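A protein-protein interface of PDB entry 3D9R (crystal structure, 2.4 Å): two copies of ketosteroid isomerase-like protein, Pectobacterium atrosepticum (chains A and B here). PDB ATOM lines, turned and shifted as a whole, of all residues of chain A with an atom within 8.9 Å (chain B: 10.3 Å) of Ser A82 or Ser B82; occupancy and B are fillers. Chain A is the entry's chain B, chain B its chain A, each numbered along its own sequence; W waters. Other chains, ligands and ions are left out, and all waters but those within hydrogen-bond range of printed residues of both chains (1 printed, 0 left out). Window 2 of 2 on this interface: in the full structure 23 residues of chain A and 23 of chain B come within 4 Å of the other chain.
The backbone carbonyl oxygen of Ser A82 sits at hydrogen-bond distance from the side-chain amide nitrogen of Gln A80, at 3.0 Å. The side-chain amide nitrogen (NE2) of Gln B80 is in hydrogen-bond range of the backbone carbonyl oxygen (O) of Ser B82 (3.0 Å). The side-chain hydroxyl of Thr A81 lies within hydrogen-bond range of the backbone carbonyl oxygen of Trp A85, at 3.5 Å. The backbone NH (N) of Phe B87 sits at hydrogen-bond distance from the backbone carbonyl oxygen (O) of Val B79. The backbone carbonyl oxygen of Trp B85 lies within hydrogen-bond range of the side-chain hydroxyl of Thr B81.
Among the printed residues, merely in contact across the chains: Thr A81 with Ser B82 (3.996 Å), Thr A81 with Trp B85 (3.6 Å), Ser A82 with Ser B82 (3.6 Å), Trp A85 with Thr B81 (3.6 Å) and Leu A114 with Phe B87 (3.4 Å).
No residue of chain B comes within 4 Å of Gln A80. Printed residues of chain B within 4 Å of Thr A81: Ser B82 and Trp B85. Of chain B, only Ser B82 (3.6 Å) comes within 4 Å of Ser A82. No residue of chain B comes within 4 Å of Ala A83. Printed residues of chain B within 4 Å of Trp A85: Thr B81. Of the printed residues of chain B, Leu A114 touches Phe B87. Thr B81 touches one residue of chain A. Of the printed residues of chain A, Ser B82 touches Thr A81 (3.996 Å) and Ser A82 (3.6 Å). No residue of chain A comes within 4 Å of Ala B83. Printed residues of chain A within 4 Å of Trp B85: Thr A81. Printed residues of chain A within 4 Å of Phe B87: Leu A114 (3.4 Å). Arg B116 touches none of the printed residues of chain A. The nearest residue of chain B that does not touch Ser A82 is Thr B81 (4.1 Å).
Of the 18 printed residues of chain B, 4 touch a printed residue of chain A. Hydrophobic or aromatic side chains of chain A that line the printed part of chain B: Trp A85 and Leu A114. Among the printed residues, 5 pairs touch across the chains. Among the printed residues, no Asp or Glu carboxylate lies within 4 Å of a Lys or Arg side-chain nitrogen of the other chain.
Thr A81 touches Ser B82, but with the chains exchanged Ser A82 does not touch Thr B81 (4.1 Å). Thr A81 touches Trp B85, and with the chains exchanged Trp A85 touches Thr B81. Ser B82 touches its own counterpart, Ser A82. 16 positions are printed for both chains. Of the 5 pairs that touch across the chains among the printed residues, 3 have their exchanged pair printed and touching as well.
Water W1 lies within hydrogen-bond range of OG of Ser B82 (2.7 Å), OG1 of Thr B81 (2.7 Å), OG of Ser A82 (2.9 Å) and OG1 of Thr A81 (2.9 Å).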
ATOM      1  N   GLU A   9       7.862 -13.772 -11.748  1.00  0.00           N
ATOM      2  CA  GLU A   9       8.295 -13.710 -10.342  1.00  0.00           C
ATOM      3  C   GLU A   9       7.305 -12.901  -9.509  1.00  0.00           C
ATOM      4  O   GLU A   9       6.999 -13.288  -8.389  1.00  0.00           O
ATOM      5  CB  GLU A   9       9.722 -13.188 -10.226  1.00  0.00           C
ATOM      6  CG  GLU A   9      10.422 -13.651  -8.949  1.00  0.00           C
ATOM      7  CD  GLU A   9      10.828 -15.129  -8.927  1.00  0.00           C
ATOM      8  OE1 GLU A   9      11.329 -15.626  -9.938  1.00  0.00           O
ATOM      9  OE2 GLU A   9      10.704 -15.793  -7.877  1.00  0.00           O
ATOM     10  N   LEU A  10       6.756 -11.822 -10.067  1.00  0.00           N
ATOM     11  CA  LEU A  10       5.678 -11.071  -9.385  1.00  0.00           C
ATOM     12  C   LEU A  10       4.429 -11.939  -9.169  1.00  0.00           C
ATOM     13  O   LEU A  10       3.804 -11.855  -8.131  1.00  0.00           O
ATOM     14  CB  LEU A  10       5.317  -9.776 -10.139  1.00  0.00           C
ATOM     15  CG  LEU A  10       6.424  -8.723 -10.275  1.00  0.00           C
ATOM     16  CD1 LEU A  10       6.016  -7.619 -11.255  1.00  0.00           C
ATOM     17  CD2 LEU A  10       6.876  -8.117  -8.937  1.00  0.00           C
ATOM     18  N   ILE A  13       5.311 -14.265  -6.209  1.00  0.00           N
ATOM     19  CA  ILE A  13       5.311 -13.433  -5.010  1.00  0.00           C
ATOM     20  C   ILE A  13       3.895 -13.137  -4.514  1.00  0.00           C
ATOM     21  O   ILE A  13       3.622 -13.252  -3.314  1.00  0.00           O
ATOM     22  CB  ILE A  13       6.031 -12.056  -5.265  1.00  0.00           C
ATOM     23  CG1 ILE A  13       7.532 -12.232  -5.526  1.00  0.00           C
ATOM     24  CG2 ILE A  13       5.814 -11.108  -4.118  1.00  0.00           C
ATOM     25  CD1 ILE A  13       8.184 -11.005  -6.286  1.00  0.00           C
ATOM     26  N   VAL A  79       5.359  -5.577  -5.540  1.00  0.00           N
ATOM     27  CA  VAL A  79       6.641  -5.003  -6.002  1.00  0.00           C
ATOM     28  C   VAL A  79       7.838  -5.878  -5.577  1.00  0.00           C
ATOM     29  O   VAL A  79       7.965  -6.265  -4.427  1.00  0.00           O
ATOM     30  CB  VAL A  79       6.851  -3.547  -5.504  1.00  0.00           C
ATOM     31  CG1 VAL A  79       8.170  -2.965  -6.080  1.00  0.00           C
ATOM     32  CG2 VAL A  79       5.669  -2.654  -5.893  1.00  0.00           C
ATOM     33  N   GLN A  80       8.684  -6.223  -6.542  1.00  0.00           N
ATOM     34  CA  GLN A  80       9.903  -6.967  -6.281  1.00  0.00           C
ATOM     35  C   GLN A  80      10.998  -5.928  -6.235  1.00  0.00           C
ATOM     36  O   GLN A  80      11.157  -5.176  -7.169  1.00  0.00           O
ATOM     37  CB  GLN A  80      10.179  -8.019  -7.383  1.00  0.00           C
ATOM     38  CG  GLN A  80      11.497  -8.821  -7.146  1.00  0.00           C
ATOM     39  CD  GLN A  80      11.629 -10.091  -7.971  1.00  0.00           C
ATOM     40  OE1 GLN A  80      10.817 -10.363  -8.854  1.00  0.00           O
ATOM     41  NE2 GLN A  80      12.660 -10.885  -7.674  1.00  0.00           N
ATOM     42  N   THR A  81      11.741  -5.851  -5.144  1.00  0.00           N
ATOM     43  CA  THR A  81      12.735  -4.781  -5.001  1.00  0.00           C
ATOM     44  C   THR A  81      14.147  -5.282  -5.348  1.00  0.00           C
ATOM     45  O   THR A  81      15.030  -4.496  -5.687  1.00  0.00           O
ATOM     46  CB  THR A  81      12.661  -4.146  -3.590  1.00  0.00           C
ATOM     47  OG1 THR A  81      12.895  -5.138  -2.579  1.00  0.00           O
ATOM     48  CG2 THR A  81      11.292  -3.530  -3.365  1.00  0.00           C
ATOM     49  N   SER A  82      14.344  -6.599  -5.277  1.00  0.00           N
ATOM     50  CA  SER A  82      15.609  -7.241  -5.651  1.00  0.00           C
ATOM     51  C   SER A  82      15.358  -8.733  -5.905  1.00  0.00           C
ATOM     52  O   SER A  82      14.221  -9.208  -5.794  1.00  0.00           O
ATOM     53  CB  SER A  82      16.703  -7.009  -4.582  1.00  0.00           C
ATOM     54  OG  SER A  82      16.420  -7.665  -3.350  1.00  0.00           O
ATOM     55  N   ALA A  83      16.410  -9.462  -6.262  1.00  0.00           N
ATOM     56  CA  ALA A  83      16.306 -10.883  -6.608  1.00  0.00           C
ATOM     57  C   ALA A  83      15.572 -11.684  -5.524  1.00  0.00           C
ATOM     58  O   ALA A  83      14.749 -12.541  -5.842  1.00  0.00           O
ATOM     59  CB  ALA A  83      17.721 -11.489  -6.888  1.00  0.00           C
ATOM     60  N   ASP A  84      15.869 -11.379  -4.255  1.00  0.00           N
ATOM     61  CA  ASP A  84      15.370 -12.150  -3.104  1.00  0.00           C
ATOM     62  C   ASP A  84      14.402 -11.420  -2.180  1.00  0.00           C
ATOM     63  O   ASP A  84      14.022 -11.974  -1.162  1.00  0.00           O
ATOM     64  CB  ASP A  84      16.544 -12.631  -2.247  1.00  0.00           C
ATOM     65  CG  ASP A  84      17.427 -13.606  -2.961  1.00  0.00           C
ATOM     66  OD1 ASP A  84      16.920 -14.370  -3.806  1.00  0.00           O
ATOM     67  OD2 ASP A  84      18.634 -13.620  -2.652  1.00  0.00           O
ATOM     68  N   TRP A  85      13.998 -10.202  -2.527  1.00  0.00           N
ATOM     69  CA  TRP A  85      13.109  -9.395  -1.673  1.00  0.00           C
ATOM     70  C   TRP A  85      11.972  -8.757  -2.436  1.00  0.00           C
ATOM     71  O   TRP A  85      12.133  -8.364  -3.572  1.00  0.00           O
ATOM     72  CB  TRP A  85      13.900  -8.305  -0.953  1.00  0.00           C
ATOM     73  CG  TRP A  85      14.814  -8.883   0.082  1.00  0.00           C
ATOM     74  CD1 TRP A  85      16.120  -9.269  -0.086  1.00  0.00           C
ATOM     75  CD2 TRP A  85      14.481  -9.182   1.436  1.00  0.00           C
ATOM     76  NE1 TRP A  85      16.617  -9.775   1.081  1.00  0.00           N
ATOM     77  CE2 TRP A  85      15.637  -9.736   2.037  1.00  0.00           C
ATOM     78  CE3 TRP A  85      13.318  -9.034   2.207  1.00  0.00           C
ATOM     79  CZ2 TRP A  85      15.670 -10.123   3.378  1.00  0.00           C
ATOM     80  CZ3 TRP A  85      13.347  -9.434   3.526  1.00  0.00           C
ATOM     81  CH2 TRP A  85      14.518  -9.968   4.102  1.00  0.00           C
ATOM     82  N   ALA A  86      10.822  -8.640  -1.772  1.00  0.00           N
ATOM     83  CA  ALA A  86       9.624  -8.100  -2.380  1.00  0.00           C
ATOM     84  C   ALA A  86       8.670  -7.590  -1.289  1.00  0.00           C
ATOM     85  O   ALA A  86       8.868  -7.851  -0.103  1.00  0.00           O
ATOM     86  CB  ALA A  86       8.949  -9.156  -3.247  1.00  0.00           C
ATOM     87  N   PHE A  87       7.673  -6.819  -1.700  1.00  0.00           N
ATOM     88  CA  PHE A  87       6.559  -6.504  -0.837  1.00  0.00           C
ATOM     89  C   PHE A  87       5.228  -6.559  -1.579  1.00  0.00           C
ATOM     90  O   PHE A  87       5.150  -6.469  -2.817  1.00  0.00           O
ATOM     91  CB  PHE A  87       6.749  -5.163  -0.065  1.00  0.00           C
ATOM     92  CG  PHE A  87       6.753  -3.926  -0.931  1.00  0.00           C
ATOM     93  CD1 PHE A  87       5.567  -3.259  -1.225  1.00  0.00           C
ATOM     94  CD2 PHE A  87       7.937  -3.399  -1.407  1.00  0.00           C
ATOM     95  CE1 PHE A  87       5.561  -2.115  -2.010  1.00  0.00           C
ATOM     96  CE2 PHE A  87       7.945  -2.255  -2.201  1.00  0.00           C
ATOM     97  CZ  PHE A  87       6.753  -1.607  -2.499  1.00  0.00           C
ATOM     98  N   LEU A 114       6.432  -8.068   3.788  1.00  0.00           N
ATOM     99  CA  LEU A 114       7.792  -8.003   3.280  1.00  0.00           C
ATOM    100  C   LEU A 114       8.224  -9.446   3.058  1.00  0.00           C
ATOM    101  O   LEU A 114       8.319 -10.221   4.010  1.00  0.00           O
ATOM    102  CB  LEU A 114       8.662  -7.270   4.296  1.00  0.00           C
ATOM    103  CG  LEU A 114      10.071  -6.853   3.935  1.00  0.00           C
ATOM    104  CD1 LEU A 114      10.159  -6.244   2.513  1.00  0.00           C
ATOM    105  CD2 LEU A 114      10.563  -5.893   5.050  1.00  0.00           C
ATOM    106  N   LEU A 115       8.462  -9.819   1.802  1.00  0.00           N
ATOM    107  CA  LEU A 115       8.737 -11.198   1.457  1.00  0.00           C
ATOM    108  C   LEU A 115      10.206 -11.421   1.101  1.00  0.00           C
ATOM    109  O   LEU A 115      10.855 -10.554   0.509  1.00  0.00           O
ATOM    110  CB  LEU A 115       7.789 -11.681   0.330  1.00  0.00           C
ATOM    111  CG  LEU A 115       6.262 -11.733   0.606  1.00  0.00           C
ATOM    112  CD1 LEU A 115       5.539 -10.685  -0.185  1.00  0.00           C
ATOM    113  CD2 LEU A 115       5.661 -13.064   0.274  1.00  0.00           C
ATOM    114  N   ARG A 116      10.711 -12.600   1.486  1.00  0.00           N
ATOM    115  CA  ARG A 116      12.090 -12.986   1.227  1.00  0.00           C
ATOM    116  C   ARG A 116      12.094 -14.341   0.544  1.00  0.00           C
ATOM    117  O   ARG A 116      11.324 -15.232   0.907  1.00  0.00           O
ATOM    118  CB  ARG A 116      12.883 -13.063   2.534  1.00  0.00           C
ATOM    119  CG  ARG A 116      14.341 -13.518   2.378  1.00  0.00           C
ATOM    120  CD  ARG A 116      15.042 -13.664   3.729  1.00  0.00           C
ATOM    121  NE  ARG A 116      16.068 -14.705   3.679  1.00  0.00           N
ATOM    122  CZ  ARG A 116      15.934 -15.950   4.135  1.00  0.00           C
ATOM    123  NH1 ARG A 116      14.815 -16.358   4.721  1.00  0.00           N
ATOM    124  NH2 ARG A 116      16.946 -16.799   4.015  1.00  0.00           N
ATOM    125  N   LYS A 117      12.957 -14.482  -0.463  1.00  0.00           N
ATOM    126  CA  LYS A 117      13.077 -15.712  -1.217  1.00  0.00           C
ATOM    127  C   LYS A 117      14.044 -16.638  -0.501  1.00  0.00           C
ATOM    128  O   LYS A 117      15.217 -16.323  -0.383  1.00  0.00           O
ATOM    129  CB  LYS A 117      13.581 -15.414  -2.617  1.00  0.00           C
ATOM    130  CG  LYS A 117      13.270 -16.471  -3.639  1.00  0.00           C
ATOM    131  CD  LYS A 117      14.054 -16.194  -4.891  1.00  0.00           C
ATOM    132  CE  LYS A 117      13.494 -16.906  -6.056  1.00  0.00           C
ATOM    133  NZ  LYS A 117      14.042 -16.315  -7.279  1.00  0.00           N
ATOM    134  N   TRP A 123       9.157 -18.006  -1.720  1.00  0.00           N
ATOM    135  CA  TRP A 123       8.879 -16.722  -1.130  1.00  0.00           C
ATOM    136  C   TRP A 123       8.149 -16.952   0.181  1.00  0.00           C
ATOM    137  O   TRP A 123       7.182 -17.731   0.248  1.00  0.00           O
ATOM    138  CB  TRP A 123       8.081 -15.846  -2.079  1.00  0.00           C
ATOM    139  CG  TRP A 123       8.867 -15.395  -3.239  1.00  0.00           C
ATOM    140  CD1 TRP A 123       8.918 -15.975  -4.472  1.00  0.00           C
ATOM    141  CD2 TRP A 123       9.738 -14.264  -3.295  1.00  0.00           C
ATOM    142  NE1 TRP A 123       9.752 -15.265  -5.297  1.00  0.00           N
ATOM    143  CE2 TRP A 123      10.274 -14.211  -4.599  1.00  0.00           C
ATOM    144  CE3 TRP A 123      10.119 -13.292  -2.377  1.00  0.00           C
ATOM    145  CZ2 TRP A 123      11.156 -13.222  -5.001  1.00  0.00           C
ATOM    146  CZ3 TRP A 123      11.000 -12.304  -2.788  1.00  0.00           C
ATOM    147  CH2 TRP A 123      11.512 -12.285  -4.081  1.00  0.00           C
ATOM    148  N   GLU B   9      26.342   2.282   5.431  1.00  0.00           N
ATOM    149  CA  GLU B   9      24.998   2.580   4.939  1.00  0.00           C
ATOM    150  C   GLU B   9      23.932   2.256   5.945  1.00  0.00           C
ATOM    151  O   GLU B   9      22.928   2.942   5.980  1.00  0.00           O
ATOM    152  CB  GLU B   9      24.703   1.874   3.625  1.00  0.00           C
ATOM    153  CG  GLU B   9      25.221   2.668   2.438  1.00  0.00           C
ATOM    154  CD  GLU B   9      24.199   3.647   1.915  1.00  0.00           C
ATOM    155  OE1 GLU B   9      23.240   3.160   1.313  1.00  0.00           O
ATOM    156  OE2 GLU B   9      24.347   4.877   2.067  1.00  0.00           O
ATOM    157  N   LEU B  10      24.154   1.246   6.785  1.00  0.00           N
ATOM    158  CA  LEU B  10      23.151   0.878   7.785  1.00  0.00           C
ATOM    159  C   LEU B  10      22.858   2.028   8.748  1.00  0.00           C
ATOM    160  O   LEU B  10      21.690   2.260   9.095  1.00  0.00           O
ATOM    161  CB  LEU B  10      23.536  -0.409   8.530  1.00  0.00           C
ATOM    162  CG  LEU B  10      23.308  -1.695   7.715  1.00  0.00           C
ATOM    163  CD1 LEU B  10      23.890  -2.934   8.420  1.00  0.00           C
ATOM    164  CD2 LEU B  10      21.868  -1.912   7.436  1.00  0.00           C
ATOM    165  N   ILE B  13      20.718   4.561   6.933  1.00  0.00           N
ATOM    166  CA  ILE B  13      19.345   4.057   6.851  1.00  0.00           C
ATOM    167  C   ILE B  13      18.645   4.312   8.193  1.00  0.00           C
ATOM    168  O   ILE B  13      17.540   4.853   8.224  1.00  0.00           O
ATOM    169  CB  ILE B  13      19.312   2.540   6.494  1.00  0.00           C
ATOM    170  CG1 ILE B  13      19.882   2.285   5.080  1.00  0.00           C
ATOM    171  CG2 ILE B  13      17.905   1.982   6.623  1.00  0.00           C
ATOM    172  CD1 ILE B  13      20.422   0.854   4.864  1.00  0.00           C
ATOM    173  N   VAL B  78      17.551  -2.754  11.858  1.00  0.00           N
ATOM    174  CA  VAL B  78      17.869  -2.048  10.629  1.00  0.00           C
ATOM    175  C   VAL B  78      18.457  -3.088   9.703  1.00  0.00           C
ATOM    176  O   VAL B  78      19.432  -3.738  10.072  1.00  0.00           O
ATOM    177  CB  VAL B  78      18.901  -0.908  10.852  1.00  0.00           C
ATOM    178  CG1 VAL B  78      19.038  -0.065   9.598  1.00  0.00           C
ATOM    179  CG2 VAL B  78      18.510  -0.045  12.033  1.00  0.00           C
ATOM    180  N   VAL B  79      17.841  -3.275   8.529  1.00  0.00           N
ATOM    181  CA  VAL B  79      18.303  -4.263   7.557  1.00  0.00           C
ATOM    182  C   VAL B  79      18.370  -3.683   6.136  1.00  0.00           C
ATOM    183  O   VAL B  79      17.407  -3.112   5.656  1.00  0.00           O
ATOM    184  CB  VAL B  79      17.418  -5.535   7.570  1.00  0.00           C
ATOM    185  CG1 VAL B  79      17.891  -6.545   6.520  1.00  0.00           C
ATOM    186  CG2 VAL B  79      17.428  -6.187   8.938  1.00  0.00           C
ATOM    187  N   GLN B  80      19.521  -3.825   5.474  1.00  0.00           N
ATOM    188  CA  GLN B  80      19.655  -3.457   4.067  1.00  0.00           C
ATOM    189  C   GLN B  80      19.496  -4.712   3.266  1.00  0.00           C
ATOM    190  O   GLN B  80      20.225  -5.665   3.478  1.00  0.00           O
ATOM    191  CB  GLN B  80      21.006  -2.790   3.767  1.00  0.00           C
ATOM    192  CG  GLN B  80      21.104  -2.302   2.313  1.00  0.00           C
ATOM    193  CD  GLN B  80      22.230  -1.304   2.042  1.00  0.00           C
ATOM    194  OE1 GLN B  80      23.002  -0.942   2.920  1.00  0.00           O
ATOM    195  NE2 GLN B  80      22.298  -0.843   0.810  1.00  0.00           N
ATOM    196  N   THR B  81      18.523  -4.722   2.357  1.00  0.00           N
ATOM    197  CA  THR B  81      18.181  -5.921   1.599  1.00  0.00           C
ATOM    198  C   THR B  81      18.832  -5.914   0.206  1.00  0.00           C
ATOM    199  O   THR B  81      19.128  -6.966  -0.356  1.00  0.00           O
ATOM    200  CB  THR B  81      16.656  -6.097   1.507  1.00  0.00           C
ATOM    201  OG1 THR B  81      16.066  -5.002   0.788  1.00  0.00           O
ATOM    202  CG2 THR B  81      16.055  -6.163   2.894  1.00  0.00           C
ATOM    203  N   SER B  82      19.047  -4.721  -0.339  1.00  0.00           N
ATOM    204  CA  SER B  82      19.786  -4.538  -1.579  1.00  0.00           C
ATOM    205  C   SER B  82      20.330  -3.119  -1.600  1.00  0.00           C
ATOM    206  O   SER B  82      20.121  -2.365  -0.655  1.00  0.00           O
ATOM    207  CB  SER B  82      18.893  -4.815  -2.789  1.00  0.00           C
ATOM    208  OG  SER B  82      17.769  -3.958  -2.827  1.00  0.00           O
ATOM    209  N   ALA B  83      21.030  -2.766  -2.673  1.00  0.00           N
ATOM    210  CA  ALA B  83      21.733  -1.484  -2.779  1.00  0.00           C
ATOM    211  C   ALA B  83      20.818  -0.293  -2.493  1.00  0.00           C
ATOM    212  O   ALA B  83      21.190   0.651  -1.809  1.00  0.00           O
ATOM    213  CB  ALA B  83      22.388  -1.359  -4.162  1.00  0.00           C
ATOM    214  N   ASP B  84      19.602  -0.358  -2.993  1.00  0.00           N
ATOM    215  CA  ASP B  84      18.688   0.761  -2.876  1.00  0.00           C
ATOM    216  C   ASP B  84      17.509   0.493  -1.980  1.00  0.00           C
ATOM    217  O   ASP B  84      16.628   1.322  -1.930  1.00  0.00           O
ATOM    218  CB  ASP B  84      18.180   1.143  -4.261  1.00  0.00           C
ATOM    219  CG  ASP B  84      19.291   1.558  -5.171  1.00  0.00           C
ATOM    220  OD1 ASP B  84      20.171   2.289  -4.699  1.00  0.00           O
ATOM    221  OD2 ASP B  84      19.305   1.145  -6.342  1.00  0.00           O
ATOM    222  N   TRP B  85      17.480  -0.645  -1.281  1.00  0.00           N
ATOM    223  CA  TRP B  85      16.321  -0.997  -0.440  1.00  0.00           C
ATOM    224  C   TRP B  85      16.702  -1.488   0.936  1.00  0.00           C
ATOM    225  O   TRP B  85      17.683  -2.214   1.091  1.00  0.00           O
ATOM    226  CB  TRP B  85      15.438  -2.049  -1.122  1.00  0.00           C
ATOM    227  CG  TRP B  85      14.681  -1.486  -2.271  1.00  0.00           C
ATOM    228  CD1 TRP B  85      15.079  -1.444  -3.567  1.00  0.00           C
ATOM    229  CD2 TRP B  85      13.407  -0.844  -2.218  1.00  0.00           C
ATOM    230  NE1 TRP B  85      14.129  -0.822  -4.322  1.00  0.00           N
ATOM    231  CE2 TRP B  85      13.092  -0.448  -3.512  1.00  0.00           C
ATOM    232  CE3 TRP B  85      12.495  -0.572  -1.188  1.00  0.00           C
ATOM    233  CZ2 TRP B  85      11.905   0.183  -3.819  1.00  0.00           C
ATOM    234  CZ3 TRP B  85      11.316   0.058  -1.499  1.00  0.00           C
ATOM    235  CH2 TRP B  85      11.030   0.430  -2.797  1.00  0.00           C
ATOM    236  N   ALA B  86      15.902  -1.093   1.926  1.00  0.00           N
ATOM    237  CA  ALA B  86      16.151  -1.452   3.315  1.00  0.00           C
ATOM    238  C   ALA B  86      14.850  -1.438   4.084  1.00  0.00           C
ATOM    239  O   ALA B  86      13.845  -0.869   3.627  1.00  0.00           O
ATOM    240  CB  ALA B  86      17.119  -0.479   3.945  1.00  0.00           C
ATOM    241  N   PHE B  87      14.865  -2.072   5.253  1.00  0.00           N
ATOM    242  CA  PHE B  87      13.791  -1.873   6.220  1.00  0.00           C
ATOM    243  C   PHE B  87      14.275  -1.606   7.634  1.00  0.00           C
ATOM    244  O   PHE B  87      15.383  -1.997   8.018  1.00  0.00           O
ATOM    245  CB  PHE B  87      12.776  -3.024   6.204  1.00  0.00           C
ATOM    246  CG  PHE B  87      13.295  -4.354   6.700  1.00  0.00           C
ATOM    247  CD1 PHE B  87      13.197  -4.693   8.042  1.00  0.00           C
ATOM    248  CD2 PHE B  87      13.777  -5.309   5.805  1.00  0.00           C
ATOM    249  CE1 PHE B  87      13.623  -5.927   8.495  1.00  0.00           C
ATOM    250  CE2 PHE B  87      14.201  -6.566   6.249  1.00  0.00           C
ATOM    251  CZ  PHE B  87      14.122  -6.877   7.596  1.00  0.00           C
ATOM    252  N   LEU B 115      12.391   1.563   3.247  1.00  0.00           N
ATOM    253  CA  LEU B 115      13.075   2.722   2.738  1.00  0.00           C
ATOM    254  C   LEU B 115      13.715   2.381   1.413  1.00  0.00           C
ATOM    255  O   LEU B 115      14.165   1.264   1.180  1.00  0.00           O
ATOM    256  CB  LEU B 115      14.117   3.259   3.749  1.00  0.00           C
ATOM    257  CG  LEU B 115      13.643   3.629   5.176  1.00  0.00           C
ATOM    258  CD1 LEU B 115      13.909   2.499   6.113  1.00  0.00           C
ATOM    259  CD2 LEU B 115      14.372   4.855   5.704  1.00  0.00           C
ATOM    260  N   ARG B 116      13.750   3.386   0.555  1.00  0.00           N
ATOM    261  CA  ARG B 116      14.336   3.294  -0.772  1.00  0.00           C
ATOM    262  C   ARG B 116      15.337   4.460  -0.911  1.00  0.00           C
ATOM    263  O   ARG B 116      15.033   5.594  -0.556  1.00  0.00           O
ATOM    264  CB  ARG B 116      13.213   3.381  -1.803  1.00  0.00           C
ATOM    265  CG  ARG B 116      13.613   3.427  -3.262  1.00  0.00           C
ATOM    266  CD  ARG B 116      12.385   3.744  -4.095  1.00  0.00           C
ATOM    267  NE  ARG B 116      12.748   4.114  -5.440  1.00  0.00           N
ATOM    268  CZ  ARG B 116      13.211   5.314  -5.780  1.00  0.00           C
ATOM    269  NH1 ARG B 116      13.335   6.280  -4.871  1.00  0.00           N
ATOM    270  NH2 ARG B 116      13.551   5.556  -7.043  1.00  0.00           N
ATOM    271  N   LYS B 117      16.530   4.144  -1.406  1.00  0.00           N
ATOM    272  CA  LYS B 117      17.568   5.119  -1.672  1.00  0.00           C
ATOM    273  C   LYS B 117      17.255   5.829  -2.983  1.00  0.00           C
ATOM    274  O   LYS B 117      17.013   5.168  -3.993  1.00  0.00           O
ATOM    275  CB  LYS B 117      18.909   4.399  -1.787  1.00  0.00           C
ATOM    276  CG  LYS B 117      20.171   5.277  -1.701  1.00  0.00           C
ATOM    277  CD  LYS B 117      21.350   4.509  -2.277  1.00  0.00           C
ATOM    278  CE  LYS B 117      22.646   4.798  -1.566  1.00  0.00           C
ATOM    279  NZ  LYS B 117      23.673   3.748  -1.899  1.00  0.00           N
ATOM    280  N   SER B 118      17.265   7.161  -2.975  1.00  0.00           N
ATOM    281  CA  SER B 118      16.891   7.928  -4.160  1.00  0.00           C
ATOM    282  C   SER B 118      18.031   8.002  -5.173  1.00  0.00           C
ATOM    283  O   SER B 118      19.146   7.544  -4.906  1.00  0.00           O
ATOM    284  CB  SER B 118      16.458   9.340  -3.777  1.00  0.00           C
ATOM    285  OG  SER B 118      17.591  10.119  -3.496  1.00  0.00           O
ATOM    286  N   TRP B 123      18.112   8.211   1.628  1.00  0.00           N
ATOM    287  CA  TRP B 123      17.146   7.192   2.027  1.00  0.00           C
ATOM    288  C   TRP B 123      15.826   7.835   2.404  1.00  0.00           C
ATOM    289  O   TRP B 123      15.768   8.693   3.296  1.00  0.00           O
ATOM    290  CB  TRP B 123      17.677   6.345   3.182  1.00  0.00           C
ATOM    291  CG  TRP B 123      18.771   5.445   2.733  1.00  0.00           C
ATOM    292  CD1 TRP B 123      20.098   5.719   2.740  1.00  0.00           C
ATOM    293  CD2 TRP B 123      18.630   4.145   2.147  1.00  0.00           C
ATOM    294  NE1 TRP B 123      20.806   4.667   2.229  1.00  0.00           N
ATOM    295  CE2 TRP B 123      19.935   3.679   1.857  1.00  0.00           C
ATOM    296  CE3 TRP B 123      17.533   3.320   1.861  1.00  0.00           C
ATOM    297  CZ2 TRP B 123      20.174   2.419   1.291  1.00  0.00           C
ATOM    298  CZ3 TRP B 123      17.762   2.072   1.305  1.00  0.00           C
ATOM    299  CH2 TRP B 123      19.071   1.633   1.016  1.00  0.00           C
HETATM  300  O   HOH W   1      15.714  -5.345  -1.841  1.00  0.00           O
